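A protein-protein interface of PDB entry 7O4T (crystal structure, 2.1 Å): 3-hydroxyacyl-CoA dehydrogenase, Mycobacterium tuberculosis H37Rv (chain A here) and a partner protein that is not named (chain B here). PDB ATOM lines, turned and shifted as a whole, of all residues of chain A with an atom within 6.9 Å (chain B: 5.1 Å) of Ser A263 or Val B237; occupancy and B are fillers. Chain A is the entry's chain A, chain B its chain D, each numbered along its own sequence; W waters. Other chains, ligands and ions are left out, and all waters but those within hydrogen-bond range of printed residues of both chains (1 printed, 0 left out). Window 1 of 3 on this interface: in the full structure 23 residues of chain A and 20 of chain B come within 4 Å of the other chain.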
ATOM      1  N   LEU A 258      23.407  23.043  -1.399  1.00  0.00           N
ATOM      2  CA  LEU A 258      24.281  22.225  -2.238  1.00  0.00           C
ATOM      3  C   LEU A 258      24.205  20.727  -1.945  1.00  0.00           C
ATOM      4  O   LEU A 258      24.277  19.942  -2.906  1.00  0.00           O
ATOM      5  CB  LEU A 258      25.724  22.729  -2.111  1.00  0.00           C
ATOM      6  CG  LEU A 258      26.722  22.271  -3.175  1.00  0.00           C
ATOM      7  CD1 LEU A 258      26.283  22.736  -4.554  1.00  0.00           C
ATOM      8  CD2 LEU A 258      28.113  22.792  -2.855  1.00  0.00           C
ATOM      9  N   PRO A 259      24.082  20.260  -0.695  1.00  0.00           N
ATOM     10  CA  PRO A 259      23.959  18.807  -0.478  1.00  0.00           C
ATOM     11  C   PRO A 259      22.737  18.179  -1.129  1.00  0.00           C
ATOM     12  O   PRO A 259      22.725  16.959  -1.328  1.00  0.00           O
ATOM     13  CB  PRO A 259      23.899  18.686   1.051  1.00  0.00           C
ATOM     14  CG  PRO A 259      24.634  19.871   1.540  1.00  0.00           C
ATOM     15  CD  PRO A 259      24.285  20.973   0.581  1.00  0.00           C
ATOM     16  N   SER A 260      21.712  18.963  -1.464  1.00  0.00           N
ATOM     17  CA  SER A 260      20.513  18.409  -2.081  1.00  0.00           C
ATOM     18  C   SER A 260      20.634  18.253  -3.591  1.00  0.00           C
ATOM     19  O   SER A 260      19.757  17.629  -4.202  1.00  0.00           O
ATOM     20  CB  SER A 260      19.301  19.286  -1.757  1.00  0.00           C
ATOM     21  OG  SER A 260      19.423  20.565  -2.355  1.00  0.00           O
ATOM     22  N   PHE A 261      21.687  18.802  -4.211  1.00  0.00           N
ATOM     23  CA  PHE A 261      21.831  18.658  -5.660  1.00  0.00           C
ATOM     24  C   PHE A 261      22.086  17.213  -6.070  1.00  0.00           C
ATOM     25  O   PHE A 261      21.385  16.720  -6.972  1.00  0.00           O
ATOM     26  CB  PHE A 261      22.928  19.594  -6.182  1.00  0.00           C
ATOM     27  CG  PHE A 261      22.564  21.053  -6.136  1.00  0.00           C
ATOM     28  CD1 PHE A 261      21.326  21.468  -5.671  1.00  0.00           C
ATOM     29  CD2 PHE A 261      23.463  22.011  -6.574  1.00  0.00           C
ATOM     30  CE1 PHE A 261      20.998  22.810  -5.632  1.00  0.00           C
ATOM     31  CE2 PHE A 261      23.140  23.354  -6.539  1.00  0.00           C
ATOM     32  CZ  PHE A 261      21.905  23.753  -6.067  1.00  0.00           C
ATOM     33  N   PRO A 262      23.041  16.480  -5.478  1.00  0.00           N
ATOM     34  CA  PRO A 262      23.233  15.085  -5.907  1.00  0.00           C
ATOM     35  C   PRO A 262      22.056  14.191  -5.573  1.00  0.00           C
ATOM     36  O   PRO A 262      21.773  13.257  -6.334  1.00  0.00           O
ATOM     37  CB  PRO A 262      24.501  14.651  -5.155  1.00  0.00           C
ATOM     38  CG  PRO A 262      25.159  15.919  -4.732  1.00  0.00           C
ATOM     39  CD  PRO A 262      24.041  16.867  -4.467  1.00  0.00           C
ATOM     40  N   SER A 263      21.361  14.443  -4.461  1.00  0.00           N
ATOM     41  CA  SER A 263      20.208  13.621  -4.109  1.00  0.00           C
ATOM     42  C   SER A 263      19.051  13.856  -5.073  1.00  0.00           C
ATOM     43  O   SER A 263      18.411  12.904  -5.533  1.00  0.00           O
ATOM     44  CB  SER A 263      19.780  13.899  -2.667  1.00  0.00           C
ATOM     45  OG  SER A 263      19.406  15.254  -2.489  1.00  0.00           O
ATOM     46  N   ASN A 264      18.766  15.123  -5.389  1.00  0.00           N
ATOM     47  CA  ASN A 264      17.725  15.420  -6.371  1.00  0.00           C
ATOM     48  C   ASN A 264      18.068  14.829  -7.733  1.00  0.00           C
ATOM     49  O   ASN A 264      17.195  14.288  -8.421  1.00  0.00           O
ATOM     50  CB  ASN A 264      17.510  16.930  -6.479  1.00  0.00           C
ATOM     51  CG  ASN A 264      16.517  17.449  -5.456  1.00  0.00           C
ATOM     52  OD1 ASN A 264      15.507  16.805  -5.176  1.00  0.00           O
ATOM     53  ND2 ASN A 264      16.803  18.616  -4.889  1.00  0.00           N
ATOM     54  N   LEU A 265      19.339  14.917  -8.137  1.00  0.00           N
ATOM     55  CA  LEU A 265      19.761  14.280  -9.379  1.00  0.00           C
ATOM     56  C   LEU A 265      19.569  12.771  -9.312  1.00  0.00           C
ATOM     57  O   LEU A 265      19.095  12.154 -10.273  1.00  0.00           O
ATOM     58  CB  LEU A 265      21.222  14.619  -9.680  1.00  0.00           C
ATOM     59  CG  LEU A 265      21.796  13.982 -10.947  1.00  0.00           C
ATOM     60  CD1 LEU A 265      21.033  14.455 -12.175  1.00  0.00           C
ATOM     61  CD2 LEU A 265      23.281  14.285 -11.087  1.00  0.00           C
ATOM     62  N   ARG A 266      19.931  12.160  -8.183  1.00  0.00           N
ATOM     63  CA  ARG A 266      19.718  10.727  -8.016  1.00  0.00           C
ATOM     64  C   ARG A 266      18.234  10.385  -7.980  1.00  0.00           C
ATOM     65  O   ARG A 266      17.835   9.304  -8.429  1.00  0.00           O
ATOM     66  CB  ARG A 266      20.415  10.241  -6.746  1.00  0.00           C
ATOM     67  CG  ARG A 266      20.392   8.740  -6.563  1.00  0.00           C
ATOM     68  CD  ARG A 266      21.612   8.266  -5.800  1.00  0.00           C
ATOM     69  NE  ARG A 266      21.784   6.822  -5.916  1.00  0.00           N
ATOM     70  CZ  ARG A 266      22.917   6.184  -5.653  1.00  0.00           C
ATOM     71  NH1 ARG A 266      23.986   6.865  -5.264  1.00  0.00           N
ATOM     72  NH2 ARG A 266      22.985   4.867  -5.786  1.00  0.00           N
ATOM     73  N   LYS A 267      17.409  11.288  -7.446  1.00  0.00           N
ATOM     74  CA  LYS A 267      15.962  11.102  -7.501  1.00  0.00           C
ATOM     75  C   LYS A 267      15.451  11.176  -8.935  1.00  0.00           C
ATOM     76  O   LYS A 267      14.614  10.363  -9.344  1.00  0.00           O
ATOM     77  CB  LYS A 267      15.276  12.149  -6.625  1.00  0.00           C
ATOM     78  CG  LYS A 267      13.758  12.151  -6.689  1.00  0.00           C
ATOM     79  CD  LYS A 267      13.197  13.254  -5.801  1.00  0.00           C
ATOM     80  CE  LYS A 267      11.684  13.175  -5.668  1.00  0.00           C
ATOM     81  NZ  LYS A 267      10.985  13.535  -6.929  1.00  0.00           N
ATOM     82  N   GLN A 268      15.951  12.139  -9.718  1.00  0.00           N
ATOM     83  CA  GLN A 268      15.503  12.279 -11.102  1.00  0.00           C
ATOM     84  C   GLN A 268      15.901  11.069 -11.939  1.00  0.00           C
ATOM     85  O   GLN A 268      15.101  10.568 -12.737  1.00  0.00           O
ATOM     86  CB  GLN A 268      16.070  13.562 -11.712  1.00  0.00           C
ATOM     87  CG  GLN A 268      15.570  14.851 -11.070  1.00  0.00           C
ATOM     88  CD  GLN A 268      14.171  15.237 -11.519  1.00  0.00           C
ATOM     89  OE1 GLN A 268      13.223  14.463 -11.380  1.00  0.00           O
ATOM     90  NE2 GLN A 268      14.037  16.443 -12.062  1.00  0.00           N
ATOM     91  N   LEU A 269      17.131  10.582 -11.768  1.00  0.00           N
ATOM     92  CA  LEU A 269      17.593   9.414 -12.505  1.00  0.00           C
ATOM     93  C   LEU A 269      17.092   8.103 -11.915  1.00  0.00           C
ATOM     94  O   LEU A 269      17.306   7.050 -12.525  1.00  0.00           O
ATOM     95  CB  LEU A 269      19.123   9.398 -12.557  1.00  0.00           C
ATOM     96  CG  LEU A 269      19.784  10.588 -13.255  1.00  0.00           C
ATOM     97  CD1 LEU A 269      21.295  10.404 -13.312  1.00  0.00           C
ATOM     98  CD2 LEU A 269      19.206  10.780 -14.645  1.00  0.00           C
ATOM     99  N   LEU A 281      27.762  17.352 -12.867  1.00  0.00           N
ATOM    100  CA  LEU A 281      27.549  18.052 -11.604  1.00  0.00           C
ATOM    101  C   LEU A 281      28.848  18.170 -10.818  1.00  0.00           C
ATOM    102  O   LEU A 281      29.165  19.234 -10.272  1.00  0.00           O
ATOM    103  CB  LEU A 281      26.484  17.330 -10.779  1.00  0.00           C
ATOM    104  CG  LEU A 281      26.095  17.986  -9.453  1.00  0.00           C
ATOM    105  CD1 LEU A 281      25.539  19.382  -9.692  1.00  0.00           C
ATOM    106  CD2 LEU A 281      25.090  17.126  -8.706  1.00  0.00           C
ATOM    107  N   ASN B 141      29.079  12.711  -2.382  1.00  0.00           N
ATOM    108  CA  ASN B 141      27.675  12.652  -1.983  1.00  0.00           C
ATOM    109  C   ASN B 141      26.922  11.590  -2.774  1.00  0.00           C
ATOM    110  O   ASN B 141      26.132  10.824  -2.209  1.00  0.00           O
ATOM    111  CB  ASN B 141      27.035  14.031  -2.177  1.00  0.00           C
ATOM    112  CG  ASN B 141      25.643  14.141  -1.568  1.00  0.00           C
ATOM    113  OD1 ASN B 141      24.815  13.238  -1.689  1.00  0.00           O
ATOM    114  ND2 ASN B 141      25.379  15.269  -0.919  1.00  0.00           N
ATOM    115  N   MET B 145      25.681   7.979  -0.943  1.00  0.00           N
ATOM    116  CA  MET B 145      24.232   8.064  -0.774  1.00  0.00           C
ATOM    117  C   MET B 145      23.882   8.824   0.505  1.00  0.00           C
ATOM    118  O   MET B 145      23.245   8.308   1.424  1.00  0.00           O
ATOM    119  CB  MET B 145      23.593   6.672  -0.792  1.00  0.00           C
ATOM    120  CG  MET B 145      23.867   5.891  -2.068  1.00  0.00           C
ATOM    121  SD  MET B 145      22.925   4.361  -2.195  1.00  0.00           S
ATOM    122  CE  MET B 145      21.269   4.999  -2.441  1.00  0.00           C
ATOM    123  N   PHE B 146      24.328  10.080   0.541  1.00  0.00           N
ATOM    124  CA  PHE B 146      24.125  10.926   1.709  1.00  0.00           C
ATOM    125  C   PHE B 146      22.640  11.128   1.980  1.00  0.00           C
ATOM    126  O   PHE B 146      21.863  11.439   1.071  1.00  0.00           O
ATOM    127  CB  PHE B 146      24.817  12.274   1.506  1.00  0.00           C
ATOM    128  CG  PHE B 146      24.469  13.300   2.548  1.00  0.00           C
ATOM    129  CD1 PHE B 146      25.068  13.272   3.795  1.00  0.00           C
ATOM    130  CD2 PHE B 146      23.547  14.299   2.275  1.00  0.00           C
ATOM    131  CE1 PHE B 146      24.749  14.217   4.754  1.00  0.00           C
ATOM    132  CE2 PHE B 146      23.224  15.246   3.229  1.00  0.00           C
ATOM    133  CZ  PHE B 146      23.827  15.204   4.471  1.00  0.00           C
ATOM    134  N   VAL B 147      22.253  10.947   3.238  1.00  0.00           N
ATOM    135  CA  VAL B 147      20.876  11.118   3.692  1.00  0.00           C
ATOM    136  C   VAL B 147      20.917  11.711   5.095  1.00  0.00           C
ATOM    137  O   VAL B 147      21.637  11.192   5.961  1.00  0.00           O
ATOM    138  CB  VAL B 147      20.109   9.785   3.665  1.00  0.00           C
ATOM    139  CG1 VAL B 147      18.969   9.808   4.662  1.00  0.00           C
ATOM    140  CG2 VAL B 147      19.581   9.500   2.266  1.00  0.00           C
ATOM    141  N   GLY B 232      14.431  17.838  -1.084  1.00  0.00           N
ATOM    142  CA  GLY B 232      15.796  17.387  -1.267  1.00  0.00           C
ATOM    143  C   GLY B 232      15.886  16.043  -1.959  1.00  0.00           C
ATOM    144  O   GLY B 232      16.954  15.656  -2.444  1.00  0.00           O
ATOM    145  N   GLY B 233      14.768  15.324  -2.014  1.00  0.00           N
ATOM    146  CA  GLY B 233      14.764  14.005  -2.614  1.00  0.00           C
ATOM    147  C   GLY B 233      15.467  12.940  -1.806  1.00  0.00           C
ATOM    148  O   GLY B 233      15.802  11.884  -2.349  1.00  0.00           O
ATOM    149  N   PHE B 234      15.699  13.185  -0.514  1.00  0.00           N
ATOM    150  CA  PHE B 234      16.428  12.228   0.309  1.00  0.00           C
ATOM    151  C   PHE B 234      15.610  10.979   0.619  1.00  0.00           C
ATOM    152  O   PHE B 234      16.196   9.925   0.889  1.00  0.00           O
ATOM    153  CB  PHE B 234      16.886  12.897   1.607  1.00  0.00           C
ATOM    154  CG  PHE B 234      17.848  14.032   1.395  1.00  0.00           C
ATOM    155  CD1 PHE B 234      19.132  13.794   0.928  1.00  0.00           C
ATOM    156  CD2 PHE B 234      17.474  15.337   1.671  1.00  0.00           C
ATOM    157  CE1 PHE B 234      20.022  14.836   0.736  1.00  0.00           C
ATOM    158  CE2 PHE B 234      18.359  16.382   1.481  1.00  0.00           C
ATOM    159  CZ  PHE B 234      19.635  16.132   1.011  1.00  0.00           C
ATOM    160  N   ASP B 235      14.278  11.070   0.591  1.00  0.00           N
ATOM    161  CA  ASP B 235      13.451   9.874   0.726  1.00  0.00           C
ATOM    162  C   ASP B 235      13.727   8.891  -0.403  1.00  0.00           C
ATOM    163  O   ASP B 235      13.930   7.694  -0.166  1.00  0.00           O
ATOM    164  CB  ASP B 235      11.970  10.257   0.750  1.00  0.00           C
ATOM    165  CG  ASP B 235      11.450  10.503   2.152  1.00  0.00           C
ATOM    166  OD1 ASP B 235      12.252  10.445   3.107  1.00  0.00           O
ATOM    167  OD2 ASP B 235      10.233  10.750   2.298  1.00  0.00           O
ATOM    168  N   ASP B 236      13.733   9.383  -1.645  1.00  0.00           N
ATOM    169  CA  ASP B 236      13.985   8.517  -2.792  1.00  0.00           C
ATOM    170  C   ASP B 236      15.377   7.902  -2.723  1.00  0.00           C
ATOM    171  O   ASP B 236      15.566   6.734  -3.083  1.00  0.00           O
ATOM    172  CB  ASP B 236      13.811   9.305  -4.091  1.00  0.00           C
ATOM    173  CG  ASP B 236      12.401   9.836  -4.269  1.00  0.00           C
ATOM    174  OD1 ASP B 236      11.958  10.649  -3.430  1.00  0.00           O
ATOM    175  OD2 ASP B 236      11.735   9.441  -5.250  1.00  0.00           O
ATOM    176  N   VAL B 237      16.364   8.675  -2.266  1.00  0.00           N
ATOM    177  CA  VAL B 237      17.724   8.154  -2.151  1.00  0.00           C
ATOM    178  C   VAL B 237      17.764   6.996  -1.164  1.00  0.00           C
ATOM    179  O   VAL B 237      18.345   5.939  -1.441  1.00  0.00           O
ATOM    180  CB  VAL B 237      18.696   9.275  -1.746  1.00  0.00           C
ATOM    181  CG1 VAL B 237      20.062   8.695  -1.400  1.00  0.00           C
ATOM    182  CG2 VAL B 237      18.811  10.308  -2.859  1.00  0.00           C
ATOM    183  N   ALA B 238      17.137   7.174   0.001  1.00  0.00           N
ATOM    184  CA  ALA B 238      17.155   6.128   1.019  1.00  0.00           C
ATOM    185  C   ALA B 238      16.447   4.870   0.536  1.00  0.00           C
ATOM    186  O   ALA B 238      16.900   3.752   0.806  1.00  0.00           O
ATOM    187  CB  ALA B 238      16.518   6.639   2.311  1.00  0.00           C
ATOM    188  N   LEU B 239      15.335   5.029  -0.188  1.00  0.00           N
ATOM    189  CA  LEU B 239      14.577   3.868  -0.632  1.00  0.00           C
ATOM    190  C   LEU B 239      15.248   3.140  -1.789  1.00  0.00           C
ATOM    191  O   LEU B 239      14.887   1.993  -2.072  1.00  0.00           O
ATOM    192  CB  LEU B 239      13.157   4.283  -1.018  1.00  0.00           C
ATOM    193  CG  LEU B 239      12.300   4.743   0.164  1.00  0.00           C
ATOM    194  CD1 LEU B 239      10.851   4.956  -0.251  1.00  0.00           C
ATOM    195  CD2 LEU B 239      12.393   3.748   1.312  1.00  0.00           C
ATOM    196  N   GLN B 240      16.211   3.771  -2.467  1.00  0.00           N
ATOM    197  CA  GLN B 240      16.976   3.055  -3.482  1.00  0.00           C
ATOM    198  C   GLN B 240      17.849   1.970  -2.860  1.00  0.00           C
ATOM    199  O   GLN B 240      18.096   0.936  -3.493  1.00  0.00           O
ATOM    200  CB  GLN B 240      17.829   4.033  -4.293  1.00  0.00           C
ATOM    201  CG  GLN B 240      17.020   4.916  -5.236  1.00  0.00           C
ATOM    202  CD  GLN B 240      17.885   5.901  -5.999  1.00  0.00           C
ATOM    203  OE1 GLN B 240      19.089   5.696  -6.155  1.00  0.00           O
ATOM    204  NE2 GLN B 240      17.274   6.981  -6.472  1.00  0.00           N
ATOM    205  N   LYS B 241      18.321   2.182  -1.631  1.00  0.00           N
ATOM    206  CA  LYS B 241      19.046   1.144  -0.906  1.00  0.00           C
ATOM    207  C   LYS B 241      18.094   0.194  -0.189  1.00  0.00           C
ATOM    208  O   LYS B 241      18.217  -1.028  -0.318  1.00  0.00           O
ATOM    209  CB  LYS B 241      20.022   1.767   0.095  1.00  0.00           C
ATOM    210  CG  LYS B 241      20.611   0.749   1.059  1.00  0.00           C
ATOM    211  CD  LYS B 241      22.098   0.956   1.275  1.00  0.00           C
ATOM    212  CE  LYS B 241      22.705  -0.233   2.001  1.00  0.00           C
ATOM    213  NZ  LYS B 241      24.182  -0.113   2.142  1.00  0.00           N
HETATM  214  O   HOH W   1      21.311   3.466  -7.181  1.00  0.00           O
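The side-chain amide nitrogen (ND2) of Asn B141 sits at hydrogen-bond distance from the backbone carbonyl oxygen (O) of Pro A259 (3.2 Å).
The side-chain hydroxyl (OG) of Ser A263 is in hydrogen-bond range of the backbone carbonyl oxygen (O) of Gly B232 (2.5 Å).
OD1 of Asn A264 sits close to O of Gly B232, at 3.3 Å.
The side-chain sulfur of Met B145 sits at hydrogen-bond distance from the guanidinium group of Arg A266 (3.6 Å).
The guanidinium group of Arg A266 sits at hydrogen-bond distance from the side-chain amide oxygen of Gln B240, at 2.9 Å.
O of Ser A260 lies within hydrogen-bond range of OG of Ser A263 (2.9 Å).
The backbone carbonyl oxygen (O) of Ser A260 is in hydrogen-bond range of the side-chain amide nitrogen (ND2) of Asn A264 (3.2 Å).
The backbone carbonyl oxygen of Asn B141 lies within hydrogen-bond range of the backbone NH of Phe B146, at 3.4 Å.
Pro A259 touches Phe B234 (O to CZ, 3.96 Å).
Gly B232 touches Ser A260.
Phe B234 touches Ser A260.
Pro A262 touches Asn B141.
Phe B234 touches Ser A263.
Ser A263 touches Val B237.
OD1 of Asn A264 touches N of Gly B233 (3.6 Å).
Lys A267 touches Gly B233.
CE of Lys A267 touches OD1 of Asp B236 (3.4 Å).
Leu A258 touches none of the printed residues of chain B.
Of the printed residues of chain B, Pro A259 touches Asn B141 and Phe B234.
Of chain B, only Gly B232 (2.5 Å), Phe B234 (3.3 Å) and Val B237 (3.7 Å) come within 4 Å of Ser A263.
Printed residues of chain B within 4 Å of Arg A266: Met B145 and Gln B240.
Of the printed residues of chain B, Lys A267 touches Gly B233 (3.6 Å) and Asp B236 (3.4 Å).
Gln A268 touches none of the printed residues of chain B.
Of the printed residues of chain A, Val B237 touches Ser A263 (3.7 Å).
The nearest residue of chain A that does not touch Val B237 is Arg A266 (4.2 Å).
Hydrophobic or aromatic side chains of chain A within 4 Å of the printed part of chain B: Pro A262.
Printed residues of chain B that touch a printed residue of chain A: Asn B141, Met B145, Gly B232, Gly B233, Phe B234, Asp B236, Val B237 and Gln B240.
Hydrophobic or aromatic side chains of chain B that line the printed part of chain A: Met B145, Phe B234 and Val B237.
Among the printed residues, no Asp or Glu carboxylate lies within 4 Å of a Lys or Arg side-chain nitrogen of the other chain.
Water W1 bridges NH2 of Arg A266 (2.6 Å) and OE1 of Gln B240 (3.3 Å).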
